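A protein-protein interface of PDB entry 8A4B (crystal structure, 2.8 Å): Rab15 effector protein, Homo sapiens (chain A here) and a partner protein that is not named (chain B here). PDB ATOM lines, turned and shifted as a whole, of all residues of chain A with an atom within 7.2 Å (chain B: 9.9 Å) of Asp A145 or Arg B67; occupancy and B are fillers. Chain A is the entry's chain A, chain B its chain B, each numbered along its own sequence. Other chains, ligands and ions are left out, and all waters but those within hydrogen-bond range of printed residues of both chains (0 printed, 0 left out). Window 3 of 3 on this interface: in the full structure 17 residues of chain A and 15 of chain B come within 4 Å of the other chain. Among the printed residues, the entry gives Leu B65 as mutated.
Of the 19 printed residues of chain B, 4 touch a printed residue of chain A. Printed residues of chain B that touch a printed residue of chain A: Arg B67, Tyr B68, Thr B70 and Ile B71. Hydrophobic or aromatic side chains of chain A that line the printed part of chain B: Ile A91, Leu A141 and Ile A142. Among the printed residues, Asp or Glu carboxylates within 4 Å of a Lys or Arg side-chain nitrogen of the other chain: Asp A145 with Arg B67 (2.7 Å).
Lys A92 touches none of the printed residues of chain B. Leu A93 touches none of the printed residues of chain B. Of chain B, only Arg B67 and Tyr B68 come within 4 Å of Gln A94. Of the printed residues of chain B, Leu A141 touches Thr B70 (3.5 Å) and Ile B71 (3.6 Å). No residue of chain B comes within 4 Å of Gly A143. Of chain B, only Arg B67 (2.7 Å) comes within 4 Å of Asp A145. No residue of chain B comes within 4 Å of Cys A146. Ala B63 touches none of the printed residues of chain A. Arg B67 touches just these residues of chain A: Ile A91, Gln A94, Ile A142 and Asp A145. Of the printed residues of chain A, Tyr B68 touches Gln A94 and Ile A142. Of the printed residues of chain A, Thr B70 touches Leu A141. The nearest residue of chain B that does not touch Asp A145 is Tyr B68 (8.4 Å). The nearest residue of chain A that does not touch Arg B67 is Leu A93 (4.5 Å). The nearest printed residue of chain B that does not touch Leu A141 is Arg B67 (5.1 Å).
Among the printed residues, pairs that only touch across the chains: Ile A91 with Arg B67, Leu A141 with Thr B70, Leu A141 with Ile B71, Ile A142 with Arg B67, Ile A142 with Tyr B68 and Ile A142 with Ile B71.
OG1 of Thr B72 sits at hydrogen-bond distance from O of Tyr B68 (2.8 Å). The backbone carbonyl oxygen (O) of Asp A145 sits at hydrogen-bond distance from the backbone NH (N) of Gln A94 (3.0 Å). The backbone NH (N) of Leu A147 lies within hydrogen-bond range of the backbone carbonyl oxygen (O) of Gln A94 (2.9 Å).
The side-chain hydroxyl of Tyr B68 sits at hydrogen-bond distance from the side-chain amide oxygen of Gln A94 (3.0 Å). The side-chain carboxylate (OD2) of Asp A145 is in salt-bridge range of the guanidinium group (NH1) of Arg B67. The side-chain amide nitrogen (NE2) of Gln A94 sits close to the guanidinium group (NH2) of Arg B67, at 3.2 Å.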
ATOM      1  N   TRP A  82     -26.752  18.379 -16.435  1.00  0.00           N
ATOM      2  CA  TRP A  82     -28.005  19.122 -16.377  1.00  0.00           C
ATOM      3  C   TRP A  82     -27.776  20.360 -15.525  1.00  0.00           C
ATOM      4  O   TRP A  82     -27.523  20.248 -14.324  1.00  0.00           O
ATOM      5  CB  TRP A  82     -29.119  18.266 -15.783  1.00  0.00           C
ATOM      6  CG  TRP A  82     -29.745  17.321 -16.746  1.00  0.00           C
ATOM      7  CD1 TRP A  82     -30.032  17.556 -18.058  1.00  0.00           C
ATOM      8  CD2 TRP A  82     -30.165  15.980 -16.477  1.00  0.00           C
ATOM      9  NE1 TRP A  82     -30.608  16.444 -18.621  1.00  0.00           N
ATOM     10  CE2 TRP A  82     -30.701  15.462 -17.671  1.00  0.00           C
ATOM     11  CE3 TRP A  82     -30.141  15.165 -15.339  1.00  0.00           C
ATOM     12  CZ2 TRP A  82     -31.207  14.167 -17.762  1.00  0.00           C
ATOM     13  CZ3 TRP A  82     -30.645  13.883 -15.430  1.00  0.00           C
ATOM     14  CH2 TRP A  82     -31.171  13.395 -16.631  1.00  0.00           C
ATOM     15  N   THR A  83     -27.866  21.537 -16.137  1.00  0.00           N
ATOM     16  CA  THR A  83     -27.768  22.791 -15.399  1.00  0.00           C
ATOM     17  C   THR A  83     -29.171  23.356 -15.221  1.00  0.00           C
ATOM     18  O   THR A  83     -29.908  23.526 -16.200  1.00  0.00           O
ATOM     19  CB  THR A  83     -26.862  23.797 -16.107  1.00  0.00           C
ATOM     20  OG1 THR A  83     -27.517  24.301 -17.275  1.00  0.00           O
ATOM     21  CG2 THR A  83     -25.558  23.139 -16.518  1.00  0.00           C
ATOM     22  N   PHE A  84     -29.538  23.618 -13.970  1.00  0.00           N
ATOM     23  CA  PHE A  84     -30.822  24.202 -13.610  1.00  0.00           C
ATOM     24  C   PHE A  84     -30.617  25.678 -13.300  1.00  0.00           C
ATOM     25  O   PHE A  84     -29.906  26.019 -12.343  1.00  0.00           O
ATOM     26  CB  PHE A  84     -31.429  23.500 -12.397  1.00  0.00           C
ATOM     27  CG  PHE A  84     -31.703  22.046 -12.607  1.00  0.00           C
ATOM     28  CD1 PHE A  84     -30.709  21.104 -12.406  1.00  0.00           C
ATOM     29  CD2 PHE A  84     -32.963  21.616 -12.985  1.00  0.00           C
ATOM     30  CE1 PHE A  84     -30.962  19.761 -12.593  1.00  0.00           C
ATOM     31  CE2 PHE A  84     -33.225  20.274 -13.171  1.00  0.00           C
ATOM     32  CZ  PHE A  84     -32.223  19.344 -12.976  1.00  0.00           C
ATOM     33  N   ILE A  91     -27.211  30.327 -12.441  1.00  0.00           N
ATOM     34  CA  ILE A  91     -27.157  28.881 -12.268  1.00  0.00           C
ATOM     35  C   ILE A  91     -27.483  28.534 -10.824  1.00  0.00           C
ATOM     36  O   ILE A  91     -26.859  29.048  -9.886  1.00  0.00           O
ATOM     37  CB  ILE A  91     -25.776  28.338 -12.664  1.00  0.00           C
ATOM     38  CG1 ILE A  91     -25.561  28.462 -14.168  1.00  0.00           C
ATOM     39  CG2 ILE A  91     -25.655  26.886 -12.256  1.00  0.00           C
ATOM     40  CD1 ILE A  91     -26.357  27.459 -14.957  1.00  0.00           C
ATOM     41  N   LYS A  92     -28.460  27.651 -10.636  1.00  0.00           N
ATOM     42  CA  LYS A  92     -28.827  27.185  -9.307  1.00  0.00           C
ATOM     43  C   LYS A  92     -28.401  25.755  -9.019  1.00  0.00           C
ATOM     44  O   LYS A  92     -28.148  25.431  -7.858  1.00  0.00           O
ATOM     45  CB  LYS A  92     -30.342  27.306  -9.098  1.00  0.00           C
ATOM     46  CG  LYS A  92     -30.867  28.732  -9.181  1.00  0.00           C
ATOM     47  CD  LYS A  92     -30.225  29.637  -8.138  1.00  0.00           C
ATOM     48  CE  LYS A  92     -30.725  31.070  -8.262  1.00  0.00           C
ATOM     49  NZ  LYS A  92     -30.047  31.986  -7.303  1.00  0.00           N
ATOM     50  N   LEU A  93     -28.312  24.890 -10.030  1.00  0.00           N
ATOM     51  CA  LEU A  93     -27.915  23.510  -9.762  1.00  0.00           C
ATOM     52  C   LEU A  93     -27.213  22.911 -10.974  1.00  0.00           C
ATOM     53  O   LEU A  93     -27.399  23.361 -12.106  1.00  0.00           O
ATOM     54  CB  LEU A  93     -29.127  22.652  -9.368  1.00  0.00           C
ATOM     55  CG  LEU A  93     -28.884  21.209  -8.915  1.00  0.00           C
ATOM     56  CD1 LEU A  93     -27.894  21.153  -7.761  1.00  0.00           C
ATOM     57  CD2 LEU A  93     -30.194  20.544  -8.533  1.00  0.00           C
ATOM     58  N   GLN A  94     -26.407  21.876 -10.728  1.00  0.00           N
ATOM     59  CA  GLN A  94     -25.768  21.125 -11.806  1.00  0.00           C
ATOM     60  C   GLN A  94     -25.643  19.663 -11.406  1.00  0.00           C
ATOM     61  O   GLN A  94     -24.973  19.342 -10.418  1.00  0.00           O
ATOM     62  CB  GLN A  94     -24.395  21.701 -12.153  1.00  0.00           C
ATOM     63  CG  GLN A  94     -24.439  22.851 -13.144  1.00  0.00           C
ATOM     64  CD  GLN A  94     -23.064  23.241 -13.657  1.00  0.00           C
ATOM     65  OE1 GLN A  94     -22.920  23.725 -14.783  1.00  0.00           O
ATOM     66  NE2 GLN A  94     -22.046  23.034 -12.831  1.00  0.00           N
ATOM     67  N   LEU A  95     -26.272  18.786 -12.184  1.00  0.00           N
ATOM     68  CA  LEU A  95     -26.164  17.343 -12.013  1.00  0.00           C
ATOM     69  C   LEU A  95     -25.228  16.786 -13.073  1.00  0.00           C
ATOM     70  O   LEU A  95     -25.510  16.887 -14.272  1.00  0.00           O
ATOM     71  CB  LEU A  95     -27.530  16.670 -12.120  1.00  0.00           C
ATOM     72  CG  LEU A  95     -28.474  16.872 -10.942  1.00  0.00           C
ATOM     73  CD1 LEU A  95     -29.743  16.090 -11.184  1.00  0.00           C
ATOM     74  CD2 LEU A  95     -27.806  16.437  -9.649  1.00  0.00           C
ATOM     75  N   CYS A 139     -16.833  17.141  -9.603  1.00  0.00           N
ATOM     76  CA  CYS A 139     -17.844  17.769  -8.760  1.00  0.00           C
ATOM     77  C   CYS A 139     -17.225  18.579  -7.628  1.00  0.00           C
ATOM     78  O   CYS A 139     -17.793  19.601  -7.226  1.00  0.00           O
ATOM     79  CB  CYS A 139     -18.795  16.713  -8.212  1.00  0.00           C
ATOM     80  SG  CYS A 139     -19.947  16.107  -9.452  1.00  0.00           S
ATOM     81  N   LEU A 141     -14.355  20.219  -7.951  1.00  0.00           N
ATOM     82  CA  LEU A 141     -13.824  21.412  -8.600  1.00  0.00           C
ATOM     83  C   LEU A 141     -14.933  22.388  -8.974  1.00  0.00           C
ATOM     84  O   LEU A 141     -14.752  23.605  -8.869  1.00  0.00           O
ATOM     85  CB  LEU A 141     -13.016  21.014  -9.834  1.00  0.00           C
ATOM     86  CG  LEU A 141     -11.494  20.884  -9.702  1.00  0.00           C
ATOM     87  CD1 LEU A 141     -10.907  22.131  -9.068  1.00  0.00           C
ATOM     88  CD2 LEU A 141     -11.095  19.658  -8.916  1.00  0.00           C
ATOM     89  N   ILE A 142     -16.081  21.878  -9.429  1.00  0.00           N
ATOM     90  CA  ILE A 142     -17.159  22.768  -9.852  1.00  0.00           C
ATOM     91  C   ILE A 142     -17.714  23.544  -8.662  1.00  0.00           C
ATOM     92  O   ILE A 142     -17.876  24.769  -8.723  1.00  0.00           O
ATOM     93  CB  ILE A 142     -18.263  21.983 -10.579  1.00  0.00           C
ATOM     94  CG1 ILE A 142     -17.729  21.374 -11.877  1.00  0.00           C
ATOM     95  CG2 ILE A 142     -19.422  22.901 -10.906  1.00  0.00           C
ATOM     96  CD1 ILE A 142     -17.269  22.408 -12.886  1.00  0.00           C
ATOM     97  N   GLY A 143     -18.013  22.854  -7.564  1.00  0.00           N
ATOM     98  CA  GLY A 143     -18.422  23.530  -6.353  1.00  0.00           C
ATOM     99  C   GLY A 143     -19.471  22.744  -5.592  1.00  0.00           C
ATOM    100  O   GLY A 143     -19.682  21.555  -5.831  1.00  0.00           O
ATOM    101  N   GLU A 144     -20.121  23.448  -4.658  1.00  0.00           N
ATOM    102  CA  GLU A 144     -21.081  22.816  -3.756  1.00  0.00           C
ATOM    103  C   GLU A 144     -22.373  22.449  -4.474  1.00  0.00           C
ATOM    104  O   GLU A 144     -22.990  21.422  -4.163  1.00  0.00           O
ATOM    105  CB  GLU A 144     -21.380  23.741  -2.575  1.00  0.00           C
ATOM    106  CG  GLU A 144     -20.183  24.072  -1.700  1.00  0.00           C
ATOM    107  CD  GLU A 144     -20.522  25.074  -0.607  1.00  0.00           C
ATOM    108  OE1 GLU A 144     -21.437  25.898  -0.819  1.00  0.00           O
ATOM    109  OE2 GLU A 144     -19.878  25.033   0.463  1.00  0.00           O
ATOM    110  N   ASP A 145     -22.812  23.279  -5.421  1.00  0.00           N
ATOM    111  CA  ASP A 145     -24.078  23.072  -6.112  1.00  0.00           C
ATOM    112  C   ASP A 145     -23.949  22.143  -7.313  1.00  0.00           C
ATOM    113  O   ASP A 145     -24.826  22.139  -8.184  1.00  0.00           O
ATOM    114  CB  ASP A 145     -24.674  24.416  -6.543  1.00  0.00           C
ATOM    115  CG  ASP A 145     -23.747  25.208  -7.446  1.00  0.00           C
ATOM    116  OD1 ASP A 145     -22.626  24.733  -7.729  1.00  0.00           O
ATOM    117  OD2 ASP A 145     -24.143  26.314  -7.876  1.00  0.00           O
ATOM    118  N   CYS A 146     -22.874  21.364  -7.379  1.00  0.00           N
ATOM    119  CA  CYS A 146     -22.689  20.360  -8.417  1.00  0.00           C
ATOM    120  C   CYS A 146     -22.655  18.991  -7.758  1.00  0.00           C
ATOM    121  O   CYS A 146     -21.799  18.730  -6.905  1.00  0.00           O
ATOM    122  CB  CYS A 146     -21.405  20.608  -9.200  1.00  0.00           C
ATOM    123  SG  CYS A 146     -21.101  19.387 -10.479  1.00  0.00           S
ATOM    124  N   LEU A 147     -23.574  18.122  -8.163  1.00  0.00           N
ATOM    125  CA  LEU A 147     -23.711  16.801  -7.573  1.00  0.00           C
ATOM    126  C   LEU A 147     -23.594  15.732  -8.649  1.00  0.00           C
ATOM    127  O   LEU A 147     -24.172  15.858  -9.736  1.00  0.00           O
ATOM    128  CB  LEU A 147     -25.042  16.666  -6.835  1.00  0.00           C
ATOM    129  CG  LEU A 147     -25.254  17.712  -5.741  1.00  0.00           C
ATOM    130  CD1 LEU A 147     -26.645  17.589  -5.165  1.00  0.00           C
ATOM    131  CD2 LEU A 147     -24.201  17.587  -4.644  1.00  0.00           C
ATOM    132  N   LYS A 209     -29.886  23.111  -1.052  1.00  0.00           N
ATOM    133  CA  LYS A 209     -29.114  22.000  -1.607  1.00  0.00           C
ATOM    134  C   LYS A 209     -28.682  20.979  -0.552  1.00  0.00           C
ATOM    135  O   LYS A 209     -28.009  20.007  -0.907  1.00  0.00           O
ATOM    136  CB  LYS A 209     -27.876  22.514  -2.360  1.00  0.00           C
ATOM    137  CG  LYS A 209     -28.157  23.276  -3.657  1.00  0.00           C
ATOM    138  CD  LYS A 209     -28.423  24.746  -3.391  1.00  0.00           C
ATOM    139  CE  LYS A 209     -28.692  25.496  -4.678  1.00  0.00           C
ATOM    140  NZ  LYS A 209     -28.858  26.963  -4.466  1.00  0.00           N
ATOM    141  N   ARG A 213     -27.469  15.286  -1.440  1.00  0.00           N
ATOM    142  CA  ARG A 213     -26.153  15.062  -0.835  1.00  0.00           C
ATOM    143  C   ARG A 213     -26.314  14.600   0.614  1.00  0.00           C
ATOM    144  O   ARG A 213     -25.352  14.151   1.246  1.00  0.00           O
ATOM    145  CB  ARG A 213     -25.286  16.329  -0.940  1.00  0.00           C
ATOM    146  CG  ARG A 213     -23.900  16.268  -0.307  1.00  0.00           C
ATOM    147  CD  ARG A 213     -23.320  17.665  -0.151  1.00  0.00           C
ATOM    148  NE  ARG A 213     -24.172  18.501   0.685  1.00  0.00           N
ATOM    149  CZ  ARG A 213     -24.010  19.806   0.861  1.00  0.00           C
ATOM    150  NH1 ARG A 213     -23.030  20.468   0.267  1.00  0.00           N
ATOM    151  NH2 ARG A 213     -24.856  20.464   1.650  1.00  0.00           N
ATOM    152  N   SER B  15     -16.276  35.182 -20.658  1.00  0.00           N
ATOM    153  CA  SER B  15     -17.275  34.476 -21.447  1.00  0.00           C
ATOM    154  C   SER B  15     -17.765  35.345 -22.602  1.00  0.00           C
ATOM    155  O   SER B  15     -17.767  36.575 -22.524  1.00  0.00           O
ATOM    156  CB  SER B  15     -18.449  34.068 -20.558  1.00  0.00           C
ATOM    157  OG  SER B  15     -19.484  33.459 -21.299  1.00  0.00           O
ATOM    158  N   SER B  37     -21.856  27.972 -25.053  1.00  0.00           N
ATOM    159  CA  SER B  37     -20.842  28.228 -24.036  1.00  0.00           C
ATOM    160  C   SER B  37     -20.198  26.925 -23.571  1.00  0.00           C
ATOM    161  O   SER B  37     -20.871  25.900 -23.410  1.00  0.00           O
ATOM    162  CB  SER B  37     -21.451  28.972 -22.849  1.00  0.00           C
ATOM    163  OG  SER B  37     -20.514  29.870 -22.285  1.00  0.00           O
ATOM    164  N   THR B  38     -18.884  26.975 -23.353  1.00  0.00           N
ATOM    165  CA  THR B  38     -18.121  25.790 -22.982  1.00  0.00           C
ATOM    166  C   THR B  38     -18.386  25.418 -21.528  1.00  0.00           C
ATOM    167  O   THR B  38     -18.399  26.283 -20.647  1.00  0.00           O
ATOM    168  CB  THR B  38     -16.626  26.027 -23.212  1.00  0.00           C
ATOM    169  OG1 THR B  38     -16.361  26.080 -24.624  1.00  0.00           O
ATOM    170  CG2 THR B  38     -15.788  24.911 -22.581  1.00  0.00           C
ATOM    171  N   VAL B  39     -18.610  24.133 -21.281  1.00  0.00           N
ATOM    172  CA  VAL B  39     -18.891  23.629 -19.943  1.00  0.00           C
ATOM    173  C   VAL B  39     -17.574  23.126 -19.364  1.00  0.00           C
ATOM    174  O   VAL B  39     -17.111  22.029 -19.684  1.00  0.00           O
ATOM    175  CB  VAL B  39     -19.964  22.540 -19.958  1.00  0.00           C
ATOM    176  CG1 VAL B  39     -20.100  21.922 -18.583  1.00  0.00           C
ATOM    177  CG2 VAL B  39     -21.290  23.130 -20.418  1.00  0.00           C
ATOM    178  N   GLY B  40     -16.966  23.937 -18.510  1.00  0.00           N
ATOM    179  CA  GLY B  40     -15.735  23.563 -17.849  1.00  0.00           C
ATOM    180  C   GLY B  40     -14.521  23.755 -18.730  1.00  0.00           C
ATOM    181  O   GLY B  40     -13.828  24.766 -18.616  1.00  0.00           O
ATOM    182  N   ILE B  41     -14.259  22.809 -19.632  1.00  0.00           N
ATOM    183  CA  ILE B  41     -13.087  22.881 -20.493  1.00  0.00           C
ATOM    184  C   ILE B  41     -13.243  21.850 -21.598  1.00  0.00           C
ATOM    185  O   ILE B  41     -13.995  20.880 -21.453  1.00  0.00           O
ATOM    186  CB  ILE B  41     -11.795  22.652 -19.661  1.00  0.00           C
ATOM    187  CG1 ILE B  41     -10.575  23.201 -20.400  1.00  0.00           C
ATOM    188  CG2 ILE B  41     -11.627  21.173 -19.318  1.00  0.00           C
ATOM    189  CD1 ILE B  41      -9.337  23.308 -19.534  1.00  0.00           C
ATOM    190  N   ALA B  63     -13.434  27.622 -20.030  1.00  0.00           N
ATOM    191  CA  ALA B  63     -14.683  28.351 -19.870  1.00  0.00           C
ATOM    192  C   ALA B  63     -14.411  29.701 -19.219  1.00  0.00           C
ATOM    193  O   ALA B  63     -13.514  29.834 -18.384  1.00  0.00           O
ATOM    194  CB  ALA B  63     -15.683  27.549 -19.035  1.00  0.00           C
ATOM    195  N   GLY B  64     -15.182  30.705 -19.615  1.00  0.00           N
ATOM    196  CA  GLY B  64     -14.933  32.051 -19.144  1.00  0.00           C
ATOM    197  C   GLY B  64     -15.712  32.436 -17.904  1.00  0.00           C
ATOM    198  O   GLY B  64     -15.415  33.456 -17.276  1.00  0.00           O
ATOM    199  N   LEU B  65     -16.718  31.642 -17.548  1.00  0.00           N
ATOM    200  CA  LEU B  65     -17.554  31.971 -16.403  1.00  0.00           C
ATOM    201  C   LEU B  65     -16.808  31.716 -15.101  1.00  0.00           C
ATOM    202  O   LEU B  65     -16.093  30.719 -14.962  1.00  0.00           O
ATOM    203  CB  LEU B  65     -18.846  31.157 -16.432  1.00  0.00           C
ATOM    204  CG  LEU B  65     -19.835  31.503 -17.545  1.00  0.00           C
ATOM    205  CD1 LEU B  65     -21.099  30.671 -17.416  1.00  0.00           C
ATOM    206  CD2 LEU B  65     -20.163  32.988 -17.523  1.00  0.00           C
ATOM    207  N   GLU B  66     -16.998  32.620 -14.135  1.00  0.00           N
ATOM    208  CA  GLU B  66     -16.365  32.463 -12.829  1.00  0.00           C
ATOM    209  C   GLU B  66     -16.702  31.114 -12.206  1.00  0.00           C
ATOM    210  O   GLU B  66     -15.884  30.545 -11.474  1.00  0.00           O
ATOM    211  CB  GLU B  66     -16.799  33.606 -11.909  1.00  0.00           C
ATOM    212  CG  GLU B  66     -16.265  33.537 -10.489  1.00  0.00           C
ATOM    213  CD  GLU B  66     -16.864  34.613  -9.600  1.00  0.00           C
ATOM    214  OE1 GLU B  66     -17.521  35.531 -10.138  1.00  0.00           O
ATOM    215  OE2 GLU B  66     -16.687  34.542  -8.364  1.00  0.00           O
ATOM    216  N   ARG B  67     -17.885  30.581 -12.514  1.00  0.00           N
ATOM    217  CA  ARG B  67     -18.311  29.300 -11.963  1.00  0.00           C
ATOM    218  C   ARG B  67     -17.303  28.190 -12.253  1.00  0.00           C
ATOM    219  O   ARG B  67     -17.075  27.312 -11.412  1.00  0.00           O
ATOM    220  CB  ARG B  67     -19.685  28.949 -12.527  1.00  0.00           C
ATOM    221  CG  ARG B  67     -20.194  27.587 -12.154  1.00  0.00           C
ATOM    222  CD  ARG B  67     -21.613  27.403 -12.646  1.00  0.00           C
ATOM    223  NE  ARG B  67     -22.192  26.178 -12.115  1.00  0.00           N
ATOM    224  CZ  ARG B  67     -22.692  26.059 -10.894  1.00  0.00           C
ATOM    225  NH1 ARG B  67     -22.712  27.081 -10.053  1.00  0.00           N
ATOM    226  NH2 ARG B  67     -23.190  24.888 -10.507  1.00  0.00           N
ATOM    227  N   TYR B  68     -16.692  28.208 -13.433  1.00  0.00           N
ATOM    228  CA  TYR B  68     -15.699  27.204 -13.790  1.00  0.00           C
ATOM    229  C   TYR B  68     -14.272  27.654 -13.509  1.00  0.00           C
ATOM    230  O   TYR B  68     -13.331  26.885 -13.753  1.00  0.00           O
ATOM    231  CB  TYR B  68     -15.845  26.817 -15.267  1.00  0.00           C
ATOM    232  CG  TYR B  68     -17.247  26.388 -15.635  1.00  0.00           C
ATOM    233  CD1 TYR B  68     -17.815  25.253 -15.072  1.00  0.00           C
ATOM    234  CD2 TYR B  68     -18.007  27.124 -16.535  1.00  0.00           C
ATOM    235  CE1 TYR B  68     -19.098  24.861 -15.397  1.00  0.00           C
ATOM    236  CE2 TYR B  68     -19.288  26.739 -16.870  1.00  0.00           C
ATOM    237  CZ  TYR B  68     -19.829  25.605 -16.298  1.00  0.00           C
ATOM    238  OH  TYR B  68     -21.107  25.217 -16.626  1.00  0.00           O
ATOM    239  N   ARG B  69     -14.085  28.860 -12.975  1.00  0.00           N
ATOM    240  CA  ARG B  69     -12.730  29.370 -12.811  1.00  0.00           C
ATOM    241  C   ARG B  69     -11.894  28.458 -11.925  1.00  0.00           C
ATOM    242  O   ARG B  69     -10.679  28.353 -12.123  1.00  0.00           O
ATOM    243  CB  ARG B  69     -12.761  30.806 -12.278  1.00  0.00           C
ATOM    244  CG  ARG B  69     -12.088  31.803 -13.246  1.00  0.00           C
ATOM    245  CD  ARG B  69     -12.601  33.244 -13.114  1.00  0.00           C
ATOM    246  NE  ARG B  69     -11.519  34.220 -13.230  1.00  0.00           N
ATOM    247  CZ  ARG B  69     -11.681  35.496 -13.566  1.00  0.00           C
ATOM    248  NH1 ARG B  69     -12.870  35.984 -13.879  1.00  0.00           N
ATOM    249  NH2 ARG B  69     -10.619  36.299 -13.596  1.00  0.00           N
ATOM    250  N   THR B  70     -12.519  27.750 -10.982  1.00  0.00           N
ATOM    251  CA  THR B  70     -11.766  26.775 -10.200  1.00  0.00           C
ATOM    252  C   THR B  70     -11.332  25.598 -11.074  1.00  0.00           C
ATOM    253  O   THR B  70     -10.132  25.313 -11.196  1.00  0.00           O
ATOM    254  CB  THR B  70     -12.590  26.299  -9.001  1.00  0.00           C
ATOM    255  OG1 THR B  70     -13.109  27.433  -8.298  1.00  0.00           O
ATOM    256  CG2 THR B  70     -11.723  25.497  -8.040  1.00  0.00           C
ATOM    257  N   ILE B  71     -12.286  24.931 -11.733  1.00  0.00           N
ATOM    258  CA  ILE B  71     -11.935  23.718 -12.475  1.00  0.00           C
ATOM    259  C   ILE B  71     -10.941  24.047 -13.584  1.00  0.00           C
ATOM    260  O   ILE B  71      -9.909  23.377 -13.738  1.00  0.00           O
ATOM    261  CB  ILE B  71     -13.196  23.008 -13.011  1.00  0.00           C
ATOM    262  CG1 ILE B  71     -12.819  21.880 -13.973  1.00  0.00           C
ATOM    263  CG2 ILE B  71     -14.137  23.966 -13.697  1.00  0.00           C
ATOM    264  CD1 ILE B  71     -12.123  20.726 -13.328  1.00  0.00           C
ATOM    265  N   THR B  72     -11.201  25.128 -14.328  1.00  0.00           N
ATOM    266  CA  THR B  72     -10.272  25.541 -15.376  1.00  0.00           C
ATOM    267  C   THR B  72      -8.869  25.732 -14.822  1.00  0.00           C
ATOM    268  O   THR B  72      -7.889  25.315 -15.451  1.00  0.00           O
ATOM    269  CB  THR B  72     -10.745  26.832 -16.047  1.00  0.00           C
ATOM    270  OG1 THR B  72     -10.993  27.831 -15.050  1.00  0.00           O
ATOM    271  CG2 THR B  72     -12.004  26.592 -16.848  1.00  0.00           C
ATOM    272  N   THR B  73      -8.748  26.336 -13.634  1.00  0.00           N
ATOM    273  CA  THR B  73      -7.413  26.604 -13.113  1.00  0.00           C
ATOM    274  C   THR B  73      -6.638  25.315 -12.902  1.00  0.00           C
ATOM    275  O   THR B  73      -5.423  25.282 -13.129  1.00  0.00           O
ATOM    276  CB  THR B  73      -7.474  27.409 -11.810  1.00  0.00           C
ATOM    277  OG1 THR B  73      -8.602  27.000 -11.025  1.00  0.00           O
ATOM    278  CG2 THR B  73      -7.556  28.903 -12.104  1.00  0.00           C
ATOM    279  N   TRP B 100      -6.708  38.129 -15.343  1.00  0.00           N
ATOM    280  CA  TRP B 100      -6.355  36.904 -16.052  1.00  0.00           C
ATOM    281  C   TRP B 100      -4.846  36.690 -16.062  1.00  0.00           C
ATOM    282  O   TRP B 100      -4.368  35.562 -15.890  1.00  0.00           O
ATOM    283  CB  TRP B 100      -6.897  36.948 -17.481  1.00  0.00           C
ATOM    284  CG  TRP B 100      -8.386  36.793 -17.594  1.00  0.00           C
ATOM    285  CD1 TRP B 100      -9.274  37.721 -18.054  1.00  0.00           C
ATOM    286  CD2 TRP B 100      -9.156  35.637 -17.255  1.00  0.00           C
ATOM    287  NE1 TRP B 100     -10.551  37.216 -18.019  1.00  0.00           N
ATOM    288  CE2 TRP B 100     -10.504  35.937 -17.533  1.00  0.00           C
ATOM    289  CE3 TRP B 100      -8.837  34.376 -16.744  1.00  0.00           C
ATOM    290  CZ2 TRP B 100     -11.531  35.024 -17.314  1.00  0.00           C
ATOM    291  CZ3 TRP B 100      -9.856  33.475 -16.525  1.00  0.00           C
ATOM    292  CH2 TRP B 100     -11.188  33.803 -16.810  1.00  0.00           C
ATOM    293  N   GLN B 103      -3.697  35.531 -12.876  1.00  0.00           N
ATOM    294  CA  GLN B 103      -4.136  34.147 -12.714  1.00  0.00           C
ATOM    295  C   GLN B 103      -3.175  33.184 -13.405  1.00  0.00           C
ATOM    296  O   GLN B 103      -2.863  32.108 -12.873  1.00  0.00           O
ATOM    297  CB  GLN B 103      -5.556  33.994 -13.252  1.00  0.00           C
ATOM    298  CG  GLN B 103      -6.183  32.650 -12.964  1.00  0.00           C
ATOM    299  CD  GLN B 103      -7.645  32.763 -12.578  1.00  0.00           C
ATOM    300  OE1 GLN B 103      -8.538  32.464 -13.375  1.00  0.00           O
ATOM    301  NE2 GLN B 103      -7.896  33.186 -11.345  1.00  0.00           N
